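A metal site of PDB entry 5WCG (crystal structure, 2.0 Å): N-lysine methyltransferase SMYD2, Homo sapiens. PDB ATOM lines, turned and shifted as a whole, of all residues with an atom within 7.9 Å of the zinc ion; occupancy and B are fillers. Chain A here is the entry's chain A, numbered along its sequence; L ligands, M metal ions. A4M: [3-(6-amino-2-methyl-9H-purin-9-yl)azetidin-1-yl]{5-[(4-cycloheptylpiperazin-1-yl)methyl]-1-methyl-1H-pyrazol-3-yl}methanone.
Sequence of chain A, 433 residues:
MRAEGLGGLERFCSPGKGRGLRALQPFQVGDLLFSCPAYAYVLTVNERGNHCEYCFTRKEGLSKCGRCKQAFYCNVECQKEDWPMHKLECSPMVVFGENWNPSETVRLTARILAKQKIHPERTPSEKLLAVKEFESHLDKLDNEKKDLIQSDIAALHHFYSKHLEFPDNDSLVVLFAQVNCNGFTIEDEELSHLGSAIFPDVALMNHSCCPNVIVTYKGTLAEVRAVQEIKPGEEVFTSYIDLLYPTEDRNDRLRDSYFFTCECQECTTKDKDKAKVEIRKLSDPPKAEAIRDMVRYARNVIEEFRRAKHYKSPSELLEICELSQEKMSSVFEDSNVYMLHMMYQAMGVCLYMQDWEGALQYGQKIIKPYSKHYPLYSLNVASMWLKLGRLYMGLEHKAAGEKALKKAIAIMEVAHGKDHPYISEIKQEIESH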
ATOM      1  N   HIS A 207     -12.327   6.161 -24.506  1.00  0.00           N
ATOM      2  CA  HIS A 207     -12.888   6.926 -23.378  1.00  0.00           C
ATOM      3  C   HIS A 207     -14.396   6.785 -23.263  1.00  0.00           C
ATOM      4  O   HIS A 207     -15.128   6.857 -24.263  1.00  0.00           O
ATOM      5  CB  HIS A 207     -12.574   8.421 -23.538  1.00  0.00           C
ATOM      6  CG  HIS A 207     -13.386   9.300 -22.660  1.00  0.00           C
ATOM      7  ND1 HIS A 207     -12.998   9.605 -21.366  1.00  0.00           N
ATOM      8  CD2 HIS A 207     -14.603   9.859 -22.833  1.00  0.00           C
ATOM      9  CE1 HIS A 207     -13.947  10.342 -20.796  1.00  0.00           C
ATOM     10  NE2 HIS A 207     -14.938  10.501 -21.665  1.00  0.00           N
ATOM     11  N   SER A 208     -14.856   6.681 -22.027  1.00  0.00           N
ATOM     12  CA  SER A 208     -16.247   6.946 -21.674  1.00  0.00           C
ATOM     13  C   SER A 208     -16.307   7.753 -20.374  1.00  0.00           C
ATOM     14  O   SER A 208     -15.437   7.590 -19.493  1.00  0.00           O
ATOM     15  CB  SER A 208     -17.040   5.650 -21.492  1.00  0.00           C
ATOM     16  OG  SER A 208     -18.350   5.931 -21.057  1.00  0.00           O
ATOM     17  N   CYS A 209     -17.328   8.574 -20.240  1.00  0.00           N
ATOM     18  CA  CYS A 209     -17.597   9.210 -18.954  1.00  0.00           C
ATOM     19  C   CYS A 209     -18.313   8.250 -17.974  1.00  0.00           C
ATOM     20  O   CYS A 209     -18.452   8.575 -16.801  1.00  0.00           O
ATOM     21  CB  CYS A 209     -18.311  10.568 -19.090  1.00  0.00           C
ATOM     22  SG  CYS A 209     -17.621  11.712 -20.319  1.00  0.00           S
ATOM     23  N   CYS A 210     -18.728   7.055 -18.426  1.00  0.00           N
ATOM     24  CA  CYS A 210     -19.087   5.951 -17.489  1.00  0.00           C
ATOM     25  C   CYS A 210     -18.212   4.765 -17.814  1.00  0.00           C
ATOM     26  O   CYS A 210     -18.650   3.812 -18.475  1.00  0.00           O
ATOM     27  CB  CYS A 210     -20.568   5.584 -17.542  1.00  0.00           C
ATOM     28  SG  CYS A 210     -21.342   6.027 -19.092  1.00  0.00           S
ATOM     29  N   ILE A 241     -10.455  11.822 -18.425  1.00  0.00           N
ATOM     30  CA  ILE A 241     -10.629  13.111 -17.742  1.00  0.00           C
ATOM     31  C   ILE A 241     -11.308  12.943 -16.392  1.00  0.00           C
ATOM     32  O   ILE A 241     -11.870  11.874 -16.098  1.00  0.00           O
ATOM     33  CB  ILE A 241     -11.462  14.075 -18.608  1.00  0.00           C
ATOM     34  CG1 ILE A 241     -12.801  13.451 -18.999  1.00  0.00           C
ATOM     35  CG2 ILE A 241     -10.704  14.465 -19.866  1.00  0.00           C
ATOM     36  CD1 ILE A 241     -13.795  14.453 -19.479  1.00  0.00           C
ATOM     37  N   LEU A 243     -14.028  13.134 -13.845  1.00  0.00           N
ATOM     38  CA  LEU A 243     -15.471  12.956 -14.021  1.00  0.00           C
ATOM     39  C   LEU A 243     -16.352  13.806 -13.085  1.00  0.00           C
ATOM     40  O   LEU A 243     -17.566  13.730 -13.151  1.00  0.00           O
ATOM     41  CB  LEU A 243     -15.832  11.463 -13.923  1.00  0.00           C
ATOM     42  CG  LEU A 243     -15.144  10.572 -14.982  1.00  0.00           C
ATOM     43  CD1 LEU A 243     -15.376   9.093 -14.716  1.00  0.00           C
ATOM     44  CD2 LEU A 243     -15.608  10.933 -16.383  1.00  0.00           C
ATOM     45  N   THR A 247     -21.116  18.128 -18.275  1.00  0.00           N
ATOM     46  CA  THR A 247     -20.874  17.653 -19.640  1.00  0.00           C
ATOM     47  C   THR A 247     -20.047  18.605 -20.486  1.00  0.00           C
ATOM     48  O   THR A 247     -19.078  18.176 -21.140  1.00  0.00           O
ATOM     49  CB  THR A 247     -22.184  17.274 -20.325  1.00  0.00           C
ATOM     50  OG1 THR A 247     -22.845  16.289 -19.512  1.00  0.00           O
ATOM     51  CG2 THR A 247     -21.919  16.693 -21.733  1.00  0.00           C
ATOM     52  N   ARG A 250     -16.344  18.599 -19.322  1.00  0.00           N
ATOM     53  CA  ARG A 250     -15.692  17.358 -19.701  1.00  0.00           C
ATOM     54  C   ARG A 250     -15.298  17.381 -21.155  1.00  0.00           C
ATOM     55  O   ARG A 250     -14.147  17.086 -21.503  1.00  0.00           O
ATOM     56  CB  ARG A 250     -16.618  16.160 -19.419  1.00  0.00           C
ATOM     57  CG  ARG A 250     -16.877  15.906 -17.923  1.00  0.00           C
ATOM     58  CD  ARG A 250     -17.434  14.525 -17.628  1.00  0.00           C
ATOM     59  NE  ARG A 250     -18.610  14.137 -18.423  1.00  0.00           N
ATOM     60  CZ  ARG A 250     -19.876  14.473 -18.158  1.00  0.00           C
ATOM     61  NH1 ARG A 250     -20.189  15.296 -17.153  1.00  0.00           N
ATOM     62  NH2 ARG A 250     -20.839  14.039 -18.958  1.00  0.00           N
ATOM     63  N   ASN A 251     -16.229  17.790 -22.008  1.00  0.00           N
ATOM     64  CA  ASN A 251     -15.983  17.862 -23.433  1.00  0.00           C
ATOM     65  C   ASN A 251     -15.039  18.984 -23.834  1.00  0.00           C
ATOM     66  O   ASN A 251     -14.311  18.828 -24.815  1.00  0.00           O
ATOM     67  CB  ASN A 251     -17.304  17.862 -24.207  1.00  0.00           C
ATOM     68  CG  ASN A 251     -17.915  16.477 -24.265  1.00  0.00           C
ATOM     69  OD1 ASN A 251     -17.387  15.612 -24.947  1.00  0.00           O
ATOM     70  ND2 ASN A 251     -18.959  16.241 -23.483  1.00  0.00           N
ATOM     71  N   LEU A 254     -11.717  17.259 -23.191  1.00  0.00           N
ATOM     72  CA  LEU A 254     -11.493  16.264 -24.262  1.00  0.00           C
ATOM     73  C   LEU A 254     -11.122  16.936 -25.584  1.00  0.00           C
ATOM     74  O   LEU A 254     -10.144  16.527 -26.239  1.00  0.00           O
ATOM     75  CB  LEU A 254     -12.691  15.324 -24.436  1.00  0.00           C
ATOM     76  CG  LEU A 254     -13.010  14.349 -23.304  1.00  0.00           C
ATOM     77  CD1 LEU A 254     -14.327  13.681 -23.595  1.00  0.00           C
ATOM     78  CD2 LEU A 254     -11.942  13.276 -23.091  1.00  0.00           C
ATOM     79  N   PHE A 260     -11.522  15.467 -29.778  1.00  0.00           N
ATOM     80  CA  PHE A 260     -12.796  14.784 -30.002  1.00  0.00           C
ATOM     81  C   PHE A 260     -13.721  15.135 -28.877  1.00  0.00           C
ATOM     82  O   PHE A 260     -13.292  15.674 -27.849  1.00  0.00           O
ATOM     83  CB  PHE A 260     -12.646  13.258 -30.126  1.00  0.00           C
ATOM     84  CG  PHE A 260     -12.385  12.521 -28.812  1.00  0.00           C
ATOM     85  CD1 PHE A 260     -11.087  12.393 -28.312  1.00  0.00           C
ATOM     86  CD2 PHE A 260     -13.441  11.941 -28.099  1.00  0.00           C
ATOM     87  CE1 PHE A 260     -10.855  11.693 -27.102  1.00  0.00           C
ATOM     88  CE2 PHE A 260     -13.211  11.282 -26.885  1.00  0.00           C
ATOM     89  CZ  PHE A 260     -11.926  11.145 -26.400  1.00  0.00           C
ATOM     90  N   THR A 261     -15.009  14.838 -29.097  1.00  0.00           N
ATOM     91  CA  THR A 261     -16.027  14.969 -28.071  1.00  0.00           C
ATOM     92  C   THR A 261     -16.758  13.657 -27.876  1.00  0.00           C
ATOM     93  O   THR A 261     -16.901  12.843 -28.801  1.00  0.00           O
ATOM     94  CB  THR A 261     -17.014  16.110 -28.378  1.00  0.00           C
ATOM     95  OG1 THR A 261     -17.591  15.910 -29.655  1.00  0.00           O
ATOM     96  CG2 THR A 261     -16.335  17.470 -28.377  1.00  0.00           C
ATOM     97  N   CYS A 262     -17.211  13.455 -26.650  1.00  0.00           N
ATOM     98  CA  CYS A 262     -17.770  12.217 -26.202  1.00  0.00           C
ATOM     99  C   CYS A 262     -19.300  12.192 -26.400  1.00  0.00           C
ATOM    100  O   CYS A 262     -19.987  13.192 -26.198  1.00  0.00           O
ATOM    101  CB  CYS A 262     -17.442  12.030 -24.710  1.00  0.00           C
ATOM    102  SG  CYS A 262     -17.925  10.438 -24.082  1.00  0.00           S
ATOM    103  N   GLU A 263     -19.796  10.999 -26.732  1.00  0.00           N
ATOM    104  CA  GLU A 263     -21.218  10.749 -26.939  1.00  0.00           C
ATOM    105  C   GLU A 263     -21.727   9.665 -26.018  1.00  0.00           C
ATOM    106  O   GLU A 263     -22.712   9.031 -26.332  1.00  0.00           O
ATOM    107  CB  GLU A 263     -21.472  10.360 -28.409  1.00  0.00           C
ATOM    108  CG  GLU A 263     -21.841  11.513 -29.316  1.00  0.00           C
ATOM    109  CD  GLU A 263     -22.561  10.990 -30.556  1.00  0.00           C
ATOM    110  OE1 GLU A 263     -21.953  10.179 -31.279  1.00  0.00           O
ATOM    111  OE2 GLU A 263     -23.752  11.330 -30.753  1.00  0.00           O
ATOM    112  N   CYS A 264     -21.093   9.454 -24.871  1.00  0.00           N
ATOM    113  CA  CYS A 264     -21.509   8.403 -23.947  1.00  0.00           C
ATOM    114  C   CYS A 264     -22.880   8.748 -23.303  1.00  0.00           C
ATOM    115  O   CYS A 264     -23.428   9.837 -23.505  1.00  0.00           O
ATOM    116  CB  CYS A 264     -20.461   8.175 -22.877  1.00  0.00           C
ATOM    117  SG  CYS A 264     -20.467   9.366 -21.514  1.00  0.00           S
ATOM    118  N   GLN A 265     -23.438   7.805 -22.546  1.00  0.00           N
ATOM    119  CA  GLN A 265     -24.758   8.004 -21.968  1.00  0.00           C
ATOM    120  C   GLN A 265     -24.830   9.220 -21.047  1.00  0.00           C
ATOM    121  O   GLN A 265     -25.843   9.940 -21.074  1.00  0.00           O
ATOM    122  CB  GLN A 265     -25.260   6.732 -21.283  1.00  0.00           C
ATOM    123  CG  GLN A 265     -24.454   6.286 -20.091  1.00  0.00           C
ATOM    124  N   GLU A 266     -23.754   9.497 -20.284  1.00  0.00           N
ATOM    125  CA  GLU A 266     -23.709  10.694 -19.427  1.00  0.00           C
ATOM    126  C   GLU A 266     -23.732  11.981 -20.225  1.00  0.00           C
ATOM    127  O   GLU A 266     -24.499  12.889 -19.884  1.00  0.00           O
ATOM    128  CB  GLU A 266     -22.479  10.712 -18.520  1.00  0.00           C
ATOM    129  CG  GLU A 266     -22.442   9.618 -17.475  1.00  0.00           C
ATOM    130  CD  GLU A 266     -23.496   9.762 -16.370  1.00  0.00           C
ATOM    131  OE1 GLU A 266     -24.290  10.749 -16.317  1.00  0.00           O
ATOM    132  OE2 GLU A 266     -23.516   8.838 -15.528  1.00  0.00           O
ATOM    133  N   CYS A 267     -22.900  12.063 -21.257  1.00  0.00           N
ATOM    134  CA  CYS A 267     -22.887  13.235 -22.133  1.00  0.00           C
ATOM    135  C   CYS A 267     -24.170  13.410 -22.952  1.00  0.00           C
ATOM    136  O   CYS A 267     -24.561  14.530 -23.216  1.00  0.00           O
ATOM    137  CB  CYS A 267     -21.683  13.238 -23.065  1.00  0.00           C
ATOM    138  SG  CYS A 267     -20.064  13.180 -22.247  1.00  0.00           S
ATOM    139  N   THR A 268     -24.781  12.294 -23.355  1.00  0.00           N
ATOM    140  CA  THR A 268     -26.028  12.292 -24.109  1.00  0.00           C
ATOM    141  C   THR A 268     -27.217  12.750 -23.250  1.00  0.00           C
ATOM    142  O   THR A 268     -27.857  13.738 -23.566  1.00  0.00           O
ATOM    143  CB  THR A 268     -26.311  10.874 -24.660  1.00  0.00           C
ATOM    144  OG1 THR A 268     -25.237  10.474 -25.528  1.00  0.00           O
ATOM    145  CG2 THR A 268     -27.623  10.840 -25.411  1.00  0.00           C
HETATM  146  C4  A4M L   1     -13.398   8.164 -27.935  1.00  0.00           C
HETATM  147  C5  A4M L   1     -11.402   7.586 -27.558  1.00  0.00           C
HETATM  148  C6  A4M L   1     -10.321   8.061 -29.836  1.00  0.00           C
HETATM  149  N1  A4M L   1     -15.296   9.131 -29.029  1.00  0.00           N
HETATM  150  C7  A4M L   1      -9.820   9.458 -30.282  1.00  0.00           C
HETATM  151  C8  A4M L   1      -7.652  10.026 -29.199  1.00  0.00           C
HETATM  152  N2  A4M L   1     -13.190   9.040 -30.174  1.00  0.00           N
HETATM  153  C9  A4M L   1      -6.541   9.616 -28.360  1.00  0.00           C
HETATM  154  C10 A4M L   1      -3.385  10.534 -27.142  1.00  0.00           C
HETATM  155  C11 A4M L   1      -5.162   8.725 -26.900  1.00  0.00           C
HETATM  156  C12 A4M L   1      -4.513   7.846 -25.859  1.00  0.00           C
HETATM  157  N3  A4M L   1     -12.572   7.604 -26.979  1.00  0.00           N
HETATM  158  C13 A4M L   1      -5.580   8.891 -23.933  1.00  0.00           C
HETATM  159  C14 A4M L   1      -5.331   9.704 -22.671  1.00  0.00           C
HETATM  160  C15 A4M L   1      -4.374   9.497 -20.381  1.00  0.00           C
HETATM  161  N4  A4M L   1     -11.403   8.078 -28.840  1.00  0.00           N
HETATM  162  O   A4M L   1      -7.567  11.153 -29.735  1.00  0.00           O
HETATM  163  N5  A4M L   1      -8.715   9.228 -29.351  1.00  0.00           N
HETATM  164  C25 A4M L   1      -8.911   7.768 -29.303  1.00  0.00           C
HETATM  165  C3  A4M L   1     -12.701   8.461 -29.084  1.00  0.00           C
HETATM  166  C1  A4M L   1     -14.496   9.348 -30.083  1.00  0.00           C
HETATM  167  C2  A4M L   1     -15.116  10.030 -31.271  1.00  0.00           C
HETATM  168  C   A4M L   1     -14.757   8.521 -27.934  1.00  0.00           C
HETATM  169  N   A4M L   1     -15.566   8.314 -26.884  1.00  0.00           N
HETATM  170  C24 A4M L   1      -6.376   8.525 -27.490  1.00  0.00           C
HETATM  171  N7  A4M L   1      -4.643   9.867 -27.420  1.00  0.00           N
HETATM  172  N6  A4M L   1      -5.474  10.430 -28.322  1.00  0.00           N
HETATM  173  N8  A4M L   1      -4.310   8.571 -24.599  1.00  0.00           N
HETATM  174  C23 A4M L   1      -3.492   7.780 -23.669  1.00  0.00           C
HETATM  175  C22 A4M L   1      -3.234   8.559 -22.383  1.00  0.00           C
HETATM  176  N9  A4M L   1      -4.515   8.924 -21.733  1.00  0.00           N
HETATM  177  C21 A4M L   1      -5.698   9.820 -19.638  1.00  0.00           C
HETATM  178  C20 A4M L   1      -5.659   9.727 -18.116  1.00  0.00           C
HETATM  179  C19 A4M L   1      -4.981  10.886 -17.398  1.00  0.00           C
HETATM  180  C18 A4M L   1      -3.542  11.156 -17.854  1.00  0.00           C
HETATM  181  C17 A4M L   1      -3.394  11.702 -19.231  1.00  0.00           C
HETATM  182  C16 A4M L   1      -3.409  10.715 -20.394  1.00  0.00           C
HETATM  183 ZN    ZN M   1     -19.080  11.178 -22.105  1.00  0.00          ZN
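N of His 207 is in hydrogen-bond range of N3 of the ligand (2.9 Å). O of His 207 is in hydrogen-bond range of N of the ligand, at 3.0 Å.
SG of Cys 267 sits close to NH2 of Arg 250, 3.5 Å away. The side-chain sulfur (SG) of Cys 267 sits close to the side-chain amide nitrogen (ND2) of Asn 251. SG of Cys 264 sits close to N of Glu 266, at 3.5 Å. The side-chain hydroxyl of Thr 268 sits at hydrogen-bond distance from the backbone carbonyl oxygen of Cys 264, 2.8 Å away. The backbone NH (N) of Cys 209 lies within hydrogen-bond range of a ring nitrogen (NE2) of His 207. SG of Cys 209 sits close to NE of Arg 250 (3.2 Å). The side-chain amide oxygen (OD1) of Asn 251 lies within hydrogen-bond range of the backbone NH (N) of Cys 262 (2.8 Å).
Along chain A the residues within 4 Å of the zinc ion span positions 209 to 267.
The zinc ion is bound by the side-chain sulfur of Cys 267 (2.2 Å), the side-chain sulfur of Cys 264 (2.4 Å), the side-chain sulfur of Cys 209 (2.4 Å) and the side-chain sulfur of Cys 262 (2.4 Å). The zinc ion has four donor atoms within binding distance.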
